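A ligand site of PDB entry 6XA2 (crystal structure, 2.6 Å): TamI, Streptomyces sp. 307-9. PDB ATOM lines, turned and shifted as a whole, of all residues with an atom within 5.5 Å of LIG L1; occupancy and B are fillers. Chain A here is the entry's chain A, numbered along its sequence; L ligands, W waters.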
ATOM      1  N   VAL A  43      11.231  16.509 -16.373  1.00  0.00           N
ATOM      2  CA  VAL A  43      10.679  16.009 -15.141  1.00  0.00           C
ATOM      3  C   VAL A  43      11.141  14.584 -15.188  1.00  0.00           C
ATOM      4  O   VAL A  43      11.004  13.907 -16.197  1.00  0.00           O
ATOM      5  CB  VAL A  43       9.165  16.239 -15.048  1.00  0.00           C
ATOM      6  CG1 VAL A  43       8.509  15.169 -14.204  1.00  0.00           C
ATOM      7  CG2 VAL A  43       8.884  17.604 -14.470  1.00  0.00           C
ATOM      8  N   PRO A  44      11.756  14.126 -14.116  1.00  0.00           N
ATOM      9  CA  PRO A  44      12.371  12.805 -14.123  1.00  0.00           C
ATOM     10  C   PRO A  44      11.671  11.571 -14.687  1.00  0.00           C
ATOM     11  O   PRO A  44      12.364  10.858 -15.389  1.00  0.00           O
ATOM     12  CB  PRO A  44      12.761  12.622 -12.679  1.00  0.00           C
ATOM     13  CG  PRO A  44      13.116  13.992 -12.251  1.00  0.00           C
ATOM     14  CD  PRO A  44      12.071  14.860 -12.881  1.00  0.00           C
ATOM     15  N   VAL A  45      10.417  11.280 -14.402  1.00  0.00           N
ATOM     16  CA  VAL A  45       9.847  10.058 -14.929  1.00  0.00           C
ATOM     17  C   VAL A  45       8.704  10.274 -15.876  1.00  0.00           C
ATOM     18  O   VAL A  45       8.601   9.618 -16.895  1.00  0.00           O
ATOM     19  CB  VAL A  45       9.460   9.094 -13.784  1.00  0.00           C
ATOM     20  CG1 VAL A  45       8.895   7.789 -14.317  1.00  0.00           C
ATOM     21  CG2 VAL A  45      10.635   8.837 -12.851  1.00  0.00           C
ATOM     22  N   CYS A  46       7.856  11.230 -15.559  1.00  0.00           N
ATOM     23  CA  CYS A  46       6.680  11.492 -16.350  1.00  0.00           C
ATOM     24  C   CYS A  46       6.854  12.626 -17.341  1.00  0.00           C
ATOM     25  O   CYS A  46       5.901  13.079 -17.936  1.00  0.00           O
ATOM     26  CB  CYS A  46       5.556  11.855 -15.409  1.00  0.00           C
ATOM     27  SG  CYS A  46       6.077  12.411 -13.798  1.00  0.00           S
ATOM     28  N   ALA A  92       9.422   6.055  -8.245  1.00  0.00           N
ATOM     29  CA  ALA A  92       8.530   5.580  -7.219  1.00  0.00           C
ATOM     30  C   ALA A  92       7.450   4.814  -7.906  1.00  0.00           C
ATOM     31  O   ALA A  92       6.521   4.361  -7.264  1.00  0.00           O
ATOM     32  CB  ALA A  92       7.963   6.756  -6.488  1.00  0.00           C
ATOM     33  N   PHE A  93       7.566   4.672  -9.205  1.00  0.00           N
ATOM     34  CA  PHE A  93       6.584   3.954  -9.981  1.00  0.00           C
ATOM     35  C   PHE A  93       7.266   2.746 -10.523  1.00  0.00           C
ATOM     36  O   PHE A  93       6.781   2.129 -11.447  1.00  0.00           O
ATOM     37  CB  PHE A  93       6.003   4.843 -11.063  1.00  0.00           C
ATOM     38  CG  PHE A  93       5.057   5.872 -10.547  1.00  0.00           C
ATOM     39  CD1 PHE A  93       3.728   5.567 -10.354  1.00  0.00           C
ATOM     40  CD2 PHE A  93       5.484   7.152 -10.254  1.00  0.00           C
ATOM     41  CE1 PHE A  93       2.846   6.508  -9.886  1.00  0.00           C
ATOM     42  CE2 PHE A  93       4.611   8.100  -9.778  1.00  0.00           C
ATOM     43  CZ  PHE A  93       3.289   7.774  -9.587  1.00  0.00           C
ATOM     44  N   HIS A 100       1.244  -1.675  -5.002  1.00  0.00           N
ATOM     45  CA  HIS A 100       0.480  -1.604  -3.765  1.00  0.00           C
ATOM     46  C   HIS A 100      -1.002  -1.322  -4.026  1.00  0.00           C
ATOM     47  O   HIS A 100      -1.450  -1.337  -5.181  1.00  0.00           O
ATOM     48  CB  HIS A 100       1.070  -0.558  -2.818  1.00  0.00           C
ATOM     49  CG  HIS A 100       1.286   0.774  -3.459  1.00  0.00           C
ATOM     50  ND1 HIS A 100       2.539   1.317  -3.628  1.00  0.00           N
ATOM     51  CD2 HIS A 100       0.416   1.696  -3.950  1.00  0.00           C
ATOM     52  CE1 HIS A 100       2.441   2.501  -4.211  1.00  0.00           C
ATOM     53  NE2 HIS A 100       1.160   2.751  -4.414  1.00  0.00           N
ATOM     54  N   LEU A 102      -2.901   1.348  -3.865  1.00  0.00           N
ATOM     55  CA  LEU A 102      -3.293   2.523  -4.640  1.00  0.00           C
ATOM     56  C   LEU A 102      -3.175   2.282  -6.135  1.00  0.00           C
ATOM     57  O   LEU A 102      -3.918   2.877  -6.917  1.00  0.00           O
ATOM     58  CB  LEU A 102      -2.447   3.725  -4.227  1.00  0.00           C
ATOM     59  CG  LEU A 102      -2.688   5.004  -5.038  1.00  0.00           C
ATOM     60  CD1 LEU A 102      -4.139   5.462  -4.939  1.00  0.00           C
ATOM     61  CD2 LEU A 102      -1.750   6.103  -4.601  1.00  0.00           C
ATOM     62  N   HIS A 103      -2.272   1.397  -6.552  1.00  0.00           N
ATOM     63  CA  HIS A 103      -2.046   1.129  -7.970  1.00  0.00           C
ATOM     64  C   HIS A 103      -2.651  -0.216  -8.374  1.00  0.00           C
ATOM     65  O   HIS A 103      -2.093  -0.937  -9.204  1.00  0.00           O
ATOM     66  CB  HIS A 103      -0.554   1.174  -8.287  1.00  0.00           C
ATOM     67  CG  HIS A 103       0.089   2.498  -8.016  1.00  0.00           C
ATOM     68  ND1 HIS A 103       1.359   2.620  -7.499  1.00  0.00           N
ATOM     69  CD2 HIS A 103      -0.376   3.767  -8.184  1.00  0.00           C
ATOM     70  CE1 HIS A 103       1.662   3.903  -7.371  1.00  0.00           C
ATOM     71  NE2 HIS A 103       0.620   4.617  -7.777  1.00  0.00           N
ATOM     72  N   LEU A 185      12.745  11.379  -4.772  1.00  0.00           N
ATOM     73  CA  LEU A 185      11.706  10.699  -5.488  1.00  0.00           C
ATOM     74  C   LEU A 185      10.655  11.643  -5.998  1.00  0.00           C
ATOM     75  O   LEU A 185      10.293  11.591  -7.158  1.00  0.00           O
ATOM     76  CB  LEU A 185      11.107   9.640  -4.594  1.00  0.00           C
ATOM     77  CG  LEU A 185      11.991   8.429  -4.290  1.00  0.00           C
ATOM     78  CD1 LEU A 185      11.485   7.698  -3.064  1.00  0.00           C
ATOM     79  CD2 LEU A 185      12.053   7.513  -5.489  1.00  0.00           C
ATOM     80  N   VAL A 186      10.095  12.454  -5.122  1.00  0.00           N
ATOM     81  CA  VAL A 186       9.069  13.425  -5.490  1.00  0.00           C
ATOM     82  C   VAL A 186       9.488  14.618  -6.290  1.00  0.00           C
ATOM     83  O   VAL A 186       8.834  14.998  -7.238  1.00  0.00           O
ATOM     84  CB  VAL A 186       8.368  13.851  -4.174  1.00  0.00           C
ATOM     85  CG1 VAL A 186       7.996  15.316  -4.146  1.00  0.00           C
ATOM     86  CG2 VAL A 186       7.196  12.945  -3.873  1.00  0.00           C
ATOM     87  N   SER A 187      10.599  15.202  -5.927  1.00  0.00           N
ATOM     88  CA  SER A 187      11.040  16.414  -6.548  1.00  0.00           C
ATOM     89  C   SER A 187      12.483  16.284  -6.873  1.00  0.00           C
ATOM     90  O   SER A 187      13.320  16.889  -6.243  1.00  0.00           O
ATOM     91  CB  SER A 187      10.896  17.525  -5.515  1.00  0.00           C
ATOM     92  OG  SER A 187      11.284  17.087  -4.219  1.00  0.00           O
ATOM     93  N   LEU A 245       4.744   2.373   0.281  1.00  0.00           N
ATOM     94  CA  LEU A 245       3.545   3.203   0.275  1.00  0.00           C
ATOM     95  C   LEU A 245       3.270   3.767   1.668  1.00  0.00           C
ATOM     96  O   LEU A 245       2.950   4.949   1.824  1.00  0.00           O
ATOM     97  CB  LEU A 245       2.359   2.392  -0.237  1.00  0.00           C
ATOM     98  CG  LEU A 245       0.963   2.992  -0.028  1.00  0.00           C
ATOM     99  CD1 LEU A 245       0.836   4.334  -0.726  1.00  0.00           C
ATOM    100  CD2 LEU A 245      -0.091   2.020  -0.522  1.00  0.00           C
ATOM    101  N   ILE A 248       6.645   6.346   2.369  1.00  0.00           N
ATOM    102  CA  ILE A 248       6.684   7.561   1.573  1.00  0.00           C
ATOM    103  C   ILE A 248       5.302   8.178   1.445  1.00  0.00           C
ATOM    104  O   ILE A 248       5.161   9.407   1.414  1.00  0.00           O
ATOM    105  CB  ILE A 248       7.310   7.265   0.198  1.00  0.00           C
ATOM    106  CG1 ILE A 248       8.728   6.726   0.389  1.00  0.00           C
ATOM    107  CG2 ILE A 248       7.318   8.506  -0.665  1.00  0.00           C
ATOM    108  CD1 ILE A 248       9.547   7.482   1.423  1.00  0.00           C
ATOM    109  N   GLY A 249       4.259   7.347   1.381  1.00  0.00           N
ATOM    110  CA  GLY A 249       2.914   7.858   1.191  1.00  0.00           C
ATOM    111  C   GLY A 249       2.470   8.787   2.299  1.00  0.00           C
ATOM    112  O   GLY A 249       1.636   9.665   2.070  1.00  0.00           O
ATOM    113  N   GLY A 250       2.966   8.588   3.507  1.00  0.00           N
ATOM    114  CA  GLY A 250       2.525   9.409   4.608  1.00  0.00           C
ATOM    115  C   GLY A 250       3.424  10.589   4.899  1.00  0.00           C
ATOM    116  O   GLY A 250       3.028  11.531   5.605  1.00  0.00           O
ATOM    117  N   GLU A 252       5.652  12.860   2.672  1.00  0.00           N
ATOM    118  CA  GLU A 252       5.621  14.102   1.897  1.00  0.00           C
ATOM    119  C   GLU A 252       4.289  14.823   2.029  1.00  0.00           C
ATOM    120  O   GLU A 252       4.224  16.056   1.886  1.00  0.00           O
ATOM    121  CB  GLU A 252       5.918  13.818   0.431  1.00  0.00           C
ATOM    122  CG  GLU A 252       7.402  13.611   0.130  1.00  0.00           C
ATOM    123  CD  GLU A 252       8.212  14.868   0.364  1.00  0.00           C
ATOM    124  OE1 GLU A 252       9.355  14.753   0.859  1.00  0.00           O
ATOM    125  OE2 GLU A 252       7.714  15.975   0.050  1.00  0.00           O
ATOM    126  N   THR A 253       3.212  14.083   2.276  1.00  0.00           N
ATOM    127  CA  THR A 253       1.879  14.693   2.370  1.00  0.00           C
ATOM    128  C   THR A 253       1.755  15.582   3.593  1.00  0.00           C
ATOM    129  O   THR A 253       1.364  16.757   3.489  1.00  0.00           O
ATOM    130  CB  THR A 253       0.841  13.591   2.430  1.00  0.00           C
ATOM    131  OG1 THR A 253       0.841  13.012   3.738  1.00  0.00           O
ATOM    132  CG2 THR A 253       1.192  12.549   1.440  1.00  0.00           C
ATOM    133  N   LEU A 296      -1.063  17.449  -2.182  1.00  0.00           N
ATOM    134  CA  LEU A 296      -1.015  16.838  -3.498  1.00  0.00           C
ATOM    135  C   LEU A 296      -1.907  17.636  -4.448  1.00  0.00           C
ATOM    136  O   LEU A 296      -3.128  17.611  -4.329  1.00  0.00           O
ATOM    137  CB  LEU A 296      -1.452  15.376  -3.433  1.00  0.00           C
ATOM    138  CG  LEU A 296      -0.442  14.442  -2.762  1.00  0.00           C
ATOM    139  CD1 LEU A 296      -1.015  13.870  -1.486  1.00  0.00           C
ATOM    140  CD2 LEU A 296      -0.043  13.338  -3.723  1.00  0.00           C
ATOM    141  N   HIS A 298      -2.199  16.865  -7.545  1.00  0.00           N
ATOM    142  CA  HIS A 298      -2.764  15.862  -8.447  1.00  0.00           C
ATOM    143  C   HIS A 298      -2.836  14.498  -7.770  1.00  0.00           C
ATOM    144  O   HIS A 298      -2.020  14.171  -6.901  1.00  0.00           O
ATOM    145  CB  HIS A 298      -1.936  15.735  -9.736  1.00  0.00           C
ATOM    146  CG  HIS A 298      -1.901  16.978 -10.566  1.00  0.00           C
ATOM    147  ND1 HIS A 298      -0.759  17.708 -10.764  1.00  0.00           N
ATOM    148  CD2 HIS A 298      -2.887  17.602 -11.272  1.00  0.00           C
ATOM    149  CE1 HIS A 298      -1.031  18.740 -11.551  1.00  0.00           C
ATOM    150  NE2 HIS A 298      -2.305  18.698 -11.863  1.00  0.00           N
ATOM    151  N   ALA A 299      -3.843  13.723  -8.156  1.00  0.00           N
ATOM    152  CA  ALA A 299      -3.962  12.309  -7.808  1.00  0.00           C
ATOM    153  C   ALA A 299      -3.076  11.460  -8.725  1.00  0.00           C
ATOM    154  O   ALA A 299      -2.481  11.962  -9.683  1.00  0.00           O
ATOM    155  CB  ALA A 299      -5.416  11.863  -7.891  1.00  0.00           C
ATOM    156  N   THR A 300      -2.997  10.153  -8.448  1.00  0.00           N
ATOM    157  CA  THR A 300      -2.224   9.283  -9.310  1.00  0.00           C
ATOM    158  C   THR A 300      -2.837   9.230 -10.710  1.00  0.00           C
ATOM    159  O   THR A 300      -4.046   9.437 -10.894  1.00  0.00           O
ATOM    160  CB  THR A 300      -2.135   7.845  -8.788  1.00  0.00           C
ATOM    161  OG1 THR A 300      -3.407   7.426  -8.279  1.00  0.00           O
ATOM    162  CG2 THR A 300      -1.074   7.700  -7.740  1.00  0.00           C
ATOM    163  N   THR A 397       9.638  21.501  -7.526  1.00  0.00           N
ATOM    164  CA  THR A 397       9.201  20.968  -8.774  1.00  0.00           C
ATOM    165  C   THR A 397       8.762  19.548  -8.640  1.00  0.00           C
ATOM    166  O   THR A 397       9.559  18.660  -8.528  1.00  0.00           O
ATOM    167  CB  THR A 397      10.246  21.149  -9.864  1.00  0.00           C
ATOM    168  OG1 THR A 397      10.569  22.543  -9.975  1.00  0.00           O
ATOM    169  CG2 THR A 397       9.735  20.663 -11.200  1.00  0.00           C
ATOM    170  N   SER A 398       7.475  19.352  -8.685  1.00  0.00           N
ATOM    171  CA  SER A 398       6.914  18.023  -8.525  1.00  0.00           C
ATOM    172  C   SER A 398       5.654  17.878  -9.362  1.00  0.00           C
ATOM    173  O   SER A 398       4.852  18.811  -9.473  1.00  0.00           O
ATOM    174  CB  SER A 398       6.577  17.732  -7.050  1.00  0.00           C
ATOM    175  OG  SER A 398       6.218  16.374  -6.879  1.00  0.00           O
ATOM    176  N   THR A 399       5.492  16.701  -9.978  1.00  0.00           N
ATOM    177  CA  THR A 399       4.300  16.438 -10.773  1.00  0.00           C
ATOM    178  C   THR A 399       3.054  16.371  -9.898  1.00  0.00           C
ATOM    179  O   THR A 399       1.972  16.821 -10.304  1.00  0.00           O
ATOM    180  CB  THR A 399       4.470  15.141 -11.568  1.00  0.00           C
ATOM    181  OG1 THR A 399       5.567  15.284 -12.476  1.00  0.00           O
ATOM    182  CG2 THR A 399       3.217  14.811 -12.353  1.00  0.00           C
ATOM    183  N   LEU A 400       3.178  15.823  -8.682  1.00  0.00           N
ATOM    184  CA  LEU A 400       2.034  15.647  -7.802  1.00  0.00           C
ATOM    185  C   LEU A 400       2.088  16.453  -6.510  1.00  0.00           C
ATOM    186  O   LEU A 400       1.021  16.748  -5.955  1.00  0.00           O
ATOM    187  CB  LEU A 400       1.867  14.164  -7.433  1.00  0.00           C
ATOM    188  CG  LEU A 400       1.946  13.161  -8.581  1.00  0.00           C
ATOM    189  CD1 LEU A 400       1.717  11.747  -8.056  1.00  0.00           C
ATOM    190  CD2 LEU A 400       0.932  13.503  -9.652  1.00  0.00           C
ATOM    191  N   ILE A 401       3.264  16.835  -6.034  1.00  0.00           N
ATOM    192  CA  ILE A 401       3.415  17.381  -4.679  1.00  0.00           C
ATOM    193  C   ILE A 401       3.416  18.898  -4.744  1.00  0.00           C
ATOM    194  O   ILE A 401       3.980  19.501  -5.683  1.00  0.00           O
ATOM    195  CB  ILE A 401       4.704  16.849  -4.018  1.00  0.00           C
ATOM    196  CG1 ILE A 401       4.488  15.409  -3.536  1.00  0.00           C
ATOM    197  CG2 ILE A 401       5.161  17.725  -2.860  1.00  0.00           C
ATOM    198  CD1 ILE A 401       3.219  15.208  -2.753  1.00  0.00           C
HETATM  199  C1  LIG L   1       1.541   9.334  -1.735  1.00  0.00           C
HETATM  200  C2  LIG L   1       0.656   8.233  -2.304  1.00  0.00           C
HETATM  201  C3  LIG L   1       2.197  10.292  -2.748  1.00  0.00           C
HETATM  202  C4  LIG L   1       1.111   8.972  -4.501  1.00  0.00           C
HETATM  203  C5  LIG L   1      -0.828   8.611  -2.377  1.00  0.00           C
HETATM  204  C6  LIG L   1       3.706  10.364  -2.506  1.00  0.00           C
HETATM  205  C7  LIG L   1      -0.264   9.585  -4.594  1.00  0.00           C
HETATM  206  C8  LIG L   1       0.678  10.156  -0.795  1.00  0.00           C
HETATM  207  C9  LIG L   1      -1.156   9.409  -3.606  1.00  0.00           C
HETATM  208  C10 LIG L   1       1.622   8.486  -5.855  1.00  0.00           C
HETATM  209  C11 LIG L   1       4.068  11.629  -1.722  1.00  0.00           C
HETATM  210  C12 LIG L   1       4.515  10.231  -3.792  1.00  0.00           C
HETATM  211  C13 LIG L   1      -0.649  10.413  -5.782  1.00  0.00           C
HETATM  212  C14 LIG L   1       4.614  11.027  -4.892  1.00  0.00           C
HETATM  213  C15 LIG L   1       3.873  12.315  -5.078  1.00  0.00           C
HETATM  214  C16 LIG L   1       5.475  10.574  -6.000  1.00  0.00           C
HETATM  215  C17 LIG L   1       5.745  11.419  -6.991  1.00  0.00           C
HETATM  216  C18 LIG L   1       6.560  11.069  -8.167  1.00  0.00           C
HETATM  217  C19 LIG L   1       7.037  12.173  -9.059  1.00  0.00           C
HETATM  218  C20 LIG L   1       8.002  12.173 -10.165  1.00  0.00           C
HETATM  219  C21 LIG L   1       8.186  13.472 -10.879  1.00  0.00           C
HETATM  220  C22 LIG L   1       6.594  13.583  -9.192  1.00  0.00           C
HETATM  221  N1  LIG L   1       7.226  14.327 -10.140  1.00  0.00           N
HETATM  222  O1  LIG L   1       1.137   7.870  -3.593  1.00  0.00           O
HETATM  223  O2  LIG L   1       1.992  10.018  -4.127  1.00  0.00           O
HETATM  224  O3  LIG L   1       6.871   9.801  -8.427  1.00  0.00           O
HETATM  225  O4  LIG L   1       8.668  11.120 -10.481  1.00  0.00           O
HETATM  226  O5  LIG L   1       5.722  14.109  -8.404  1.00  0.00           O
HETATM  227  C1  LG2 L   2      -4.235   7.627  -1.002  1.00  0.00           C
HETATM  228  C2  LG2 L   2      -3.672  12.360  -0.064  1.00  0.00           C
HETATM  229  C3  LG2 L   2      -1.612  11.323   4.196  1.00  0.00           C
HETATM  230  C4  LG2 L   2      -1.396   6.674   2.840  1.00  0.00           C
HETATM  231  C5  LG2 L   2      -4.319   9.001  -1.100  1.00  0.00           C
HETATM  232  C6  LG2 L   2      -5.046   9.757  -2.110  1.00  0.00           C
HETATM  233  C7  LG2 L   2      -4.876  11.059  -1.847  1.00  0.00           C
HETATM  234  C8  LG2 L   2      -4.064  11.181  -0.656  1.00  0.00           C
HETATM  235  C9  LG2 L   2      -5.456  12.237  -2.654  1.00  0.00           C
HETATM  236  C10 LG2 L   2      -5.834   9.157  -3.292  1.00  0.00           C
HETATM  237  C11 LG2 L   2      -5.011   9.301  -4.572  1.00  0.00           C
HETATM  238  C12 LG2 L   2      -5.817   8.846  -5.755  1.00  0.00           C
HETATM  239  O1  LG2 L   2      -5.302   8.924  -6.904  1.00  0.00           O
HETATM  240  O2  LG2 L   2      -6.990   8.427  -5.566  1.00  0.00           O
HETATM  241  C13 LG2 L   2      -3.130  12.497   1.200  1.00  0.00           C
HETATM  242  C14 LG2 L   2      -2.994  13.739   1.929  1.00  0.00           C
HETATM  243  C15 LG2 L   2      -2.419  13.458   3.119  1.00  0.00           C
HETATM  244  C16 LG2 L   2      -2.177  12.027   3.154  1.00  0.00           C
HETATM  245  C17 LG2 L   2      -3.457  15.099   1.368  1.00  0.00           C
HETATM  246  C18 LG2 L   2      -2.033  14.394   4.294  1.00  0.00           C
HETATM  247  C19 LG2 L   2      -2.165  15.724   4.272  1.00  0.00           C
HETATM  248  C20 LG2 L   2      -1.347   9.972   4.205  1.00  0.00           C
HETATM  249  C21 LG2 L   2      -0.693   9.235   5.272  1.00  0.00           C
HETATM  250  C22 LG2 L   2      -0.637   7.939   4.895  1.00  0.00           C
HETATM  251  C23 LG2 L   2      -1.250   7.833   3.585  1.00  0.00           C
HETATM  252  C24 LG2 L   2      -0.185   9.901   6.569  1.00  0.00           C
HETATM  253  C25 LG2 L   2      -0.028   6.704   5.629  1.00  0.00           C
HETATM  254  C26 LG2 L   2       0.714   6.772   6.736  1.00  0.00           C
HETATM  255  C27 LG2 L   2      -2.211   6.508   1.735  1.00  0.00           C
HETATM  256  C28 LG2 L   2      -2.617   5.244   1.149  1.00  0.00           C
HETATM  257  C29 LG2 L   2      -3.406   5.498   0.094  1.00  0.00           C
HETATM  258  C30 LG2 L   2      -3.517   6.941  -0.035  1.00  0.00           C
HETATM  259  C31 LG2 L   2      -2.223   3.850   1.671  1.00  0.00           C
HETATM  260  C32 LG2 L   2      -4.052   4.442  -0.827  1.00  0.00           C
HETATM  261  C33 LG2 L   2      -5.479   4.153  -0.355  1.00  0.00           C
HETATM  262  C34 LG2 L   2      -6.162   3.149  -1.255  1.00  0.00           C
HETATM  263  O3  LG2 L   2      -5.642   2.878  -2.377  1.00  0.00           O
HETATM  264  O4  LG2 L   2      -7.236   2.631  -0.857  1.00  0.00           O
HETATM  265  N1  LG2 L   2      -3.748   9.909  -0.232  1.00  0.00           N
HETATM  266  N2  LG2 L   2      -2.619  11.473   1.970  1.00  0.00           N
HETATM  267  N3  LG2 L   2      -1.668   9.083   3.206  1.00  0.00           N
HETATM  268  N4  LG2 L   2      -2.779   7.516   0.983  1.00  0.00           N
HETATM  269 FE1  LG2 L   2      -2.685   9.500   1.474  1.00  0.00          FE
HETATM  270  O   HOH W   1      11.222  12.807  -9.324  1.00  0.00           O
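Water W1 lies within hydrogen-bond range of the backbone carbonyl oxygen (O) of Leu 185 (2.7 Å) and an oxygen (O4) of LIG L1 (3.3 Å).
The backbone carbonyl oxygen of Val 186 lies close to a nitrogen (N1) of LIG L1. Merely in contact with LIG L1: Val 43 (3.7 Å), Val 45 (3.8 Å), Cys 46 (3.8 Å), Ala 92 (3.8 Å), Phe 93 (3.1 Å), Leu 102 (3.5 Å), Leu 185 (3.7 Å), Ile 248 (3.996 Å), Gly 249 (3.1 Å), Glu 252 (3.6 Å), Thr 253 (3.3 Å), Leu 296 (3.6 Å), Ala 299 (3.96 Å), Thr 300 (3.4 Å) and Ile 401 (3.5 Å). Hydrophobic or aromatic side chains that line LIG L1: Val 43, Val 45, Ala 92, Phe 93, Leu 102, Val 186, Leu 296, Leu 400 and Ile 401. Of the 27 residues printed, 19 come within 4 Å of LIG L1. The nearest printed residue that does not touch LIG L1 is His 298 (4.2 Å).
N of Thr 399 lies within hydrogen-bond range of N1 of LIG L1, 2.9 Å away. An oxygen (O5) of LIG L1 is in hydrogen-bond range of the backbone NH (N) of Leu 400 (3.1 Å). The side-chain hydroxyl (OG) of Ser 398 sits at hydrogen-bond distance from an oxygen (O5) of LIG L1, 2.8 Å away. The side-chain hydroxyl of Thr 399 is in hydrogen-bond range of a nitrogen (N1) of LIG L1 (3.0 Å). An oxygen (O3) of LG2 L2 lies close to the backbone NH of Leu 102, at 3.5 Å. The backbone NH of Thr 300 lies within hydrogen-bond range of an oxygen (O1) of LG2 L2, 3.0 Å away. The side-chain hydroxyl of Thr 300 sits at hydrogen-bond distance from an oxygen (O1) of LG2 L2, 2.8 Å away.
The backbone carbonyl oxygen (O) of Gly 250 is in hydrogen-bond range of the side-chain hydroxyl (OG1) of Thr 253, 3.2 Å away. A ring nitrogen (ND1) of His 298 is in hydrogen-bond range of the backbone carbonyl oxygen (O) of Thr 399, 2.9 Å away. OG of Ser 398 lies within hydrogen-bond range of O of Val 186, at 3.0 Å. The side-chain hydroxyl (OG) of Ser 398 sits at hydrogen-bond distance from the backbone NH (N) of Ile 401 (3.1 Å). The side-chain sulfur (SG) of Cys 46 is in hydrogen-bond range of the side-chain hydroxyl (OG1) of Thr 399.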
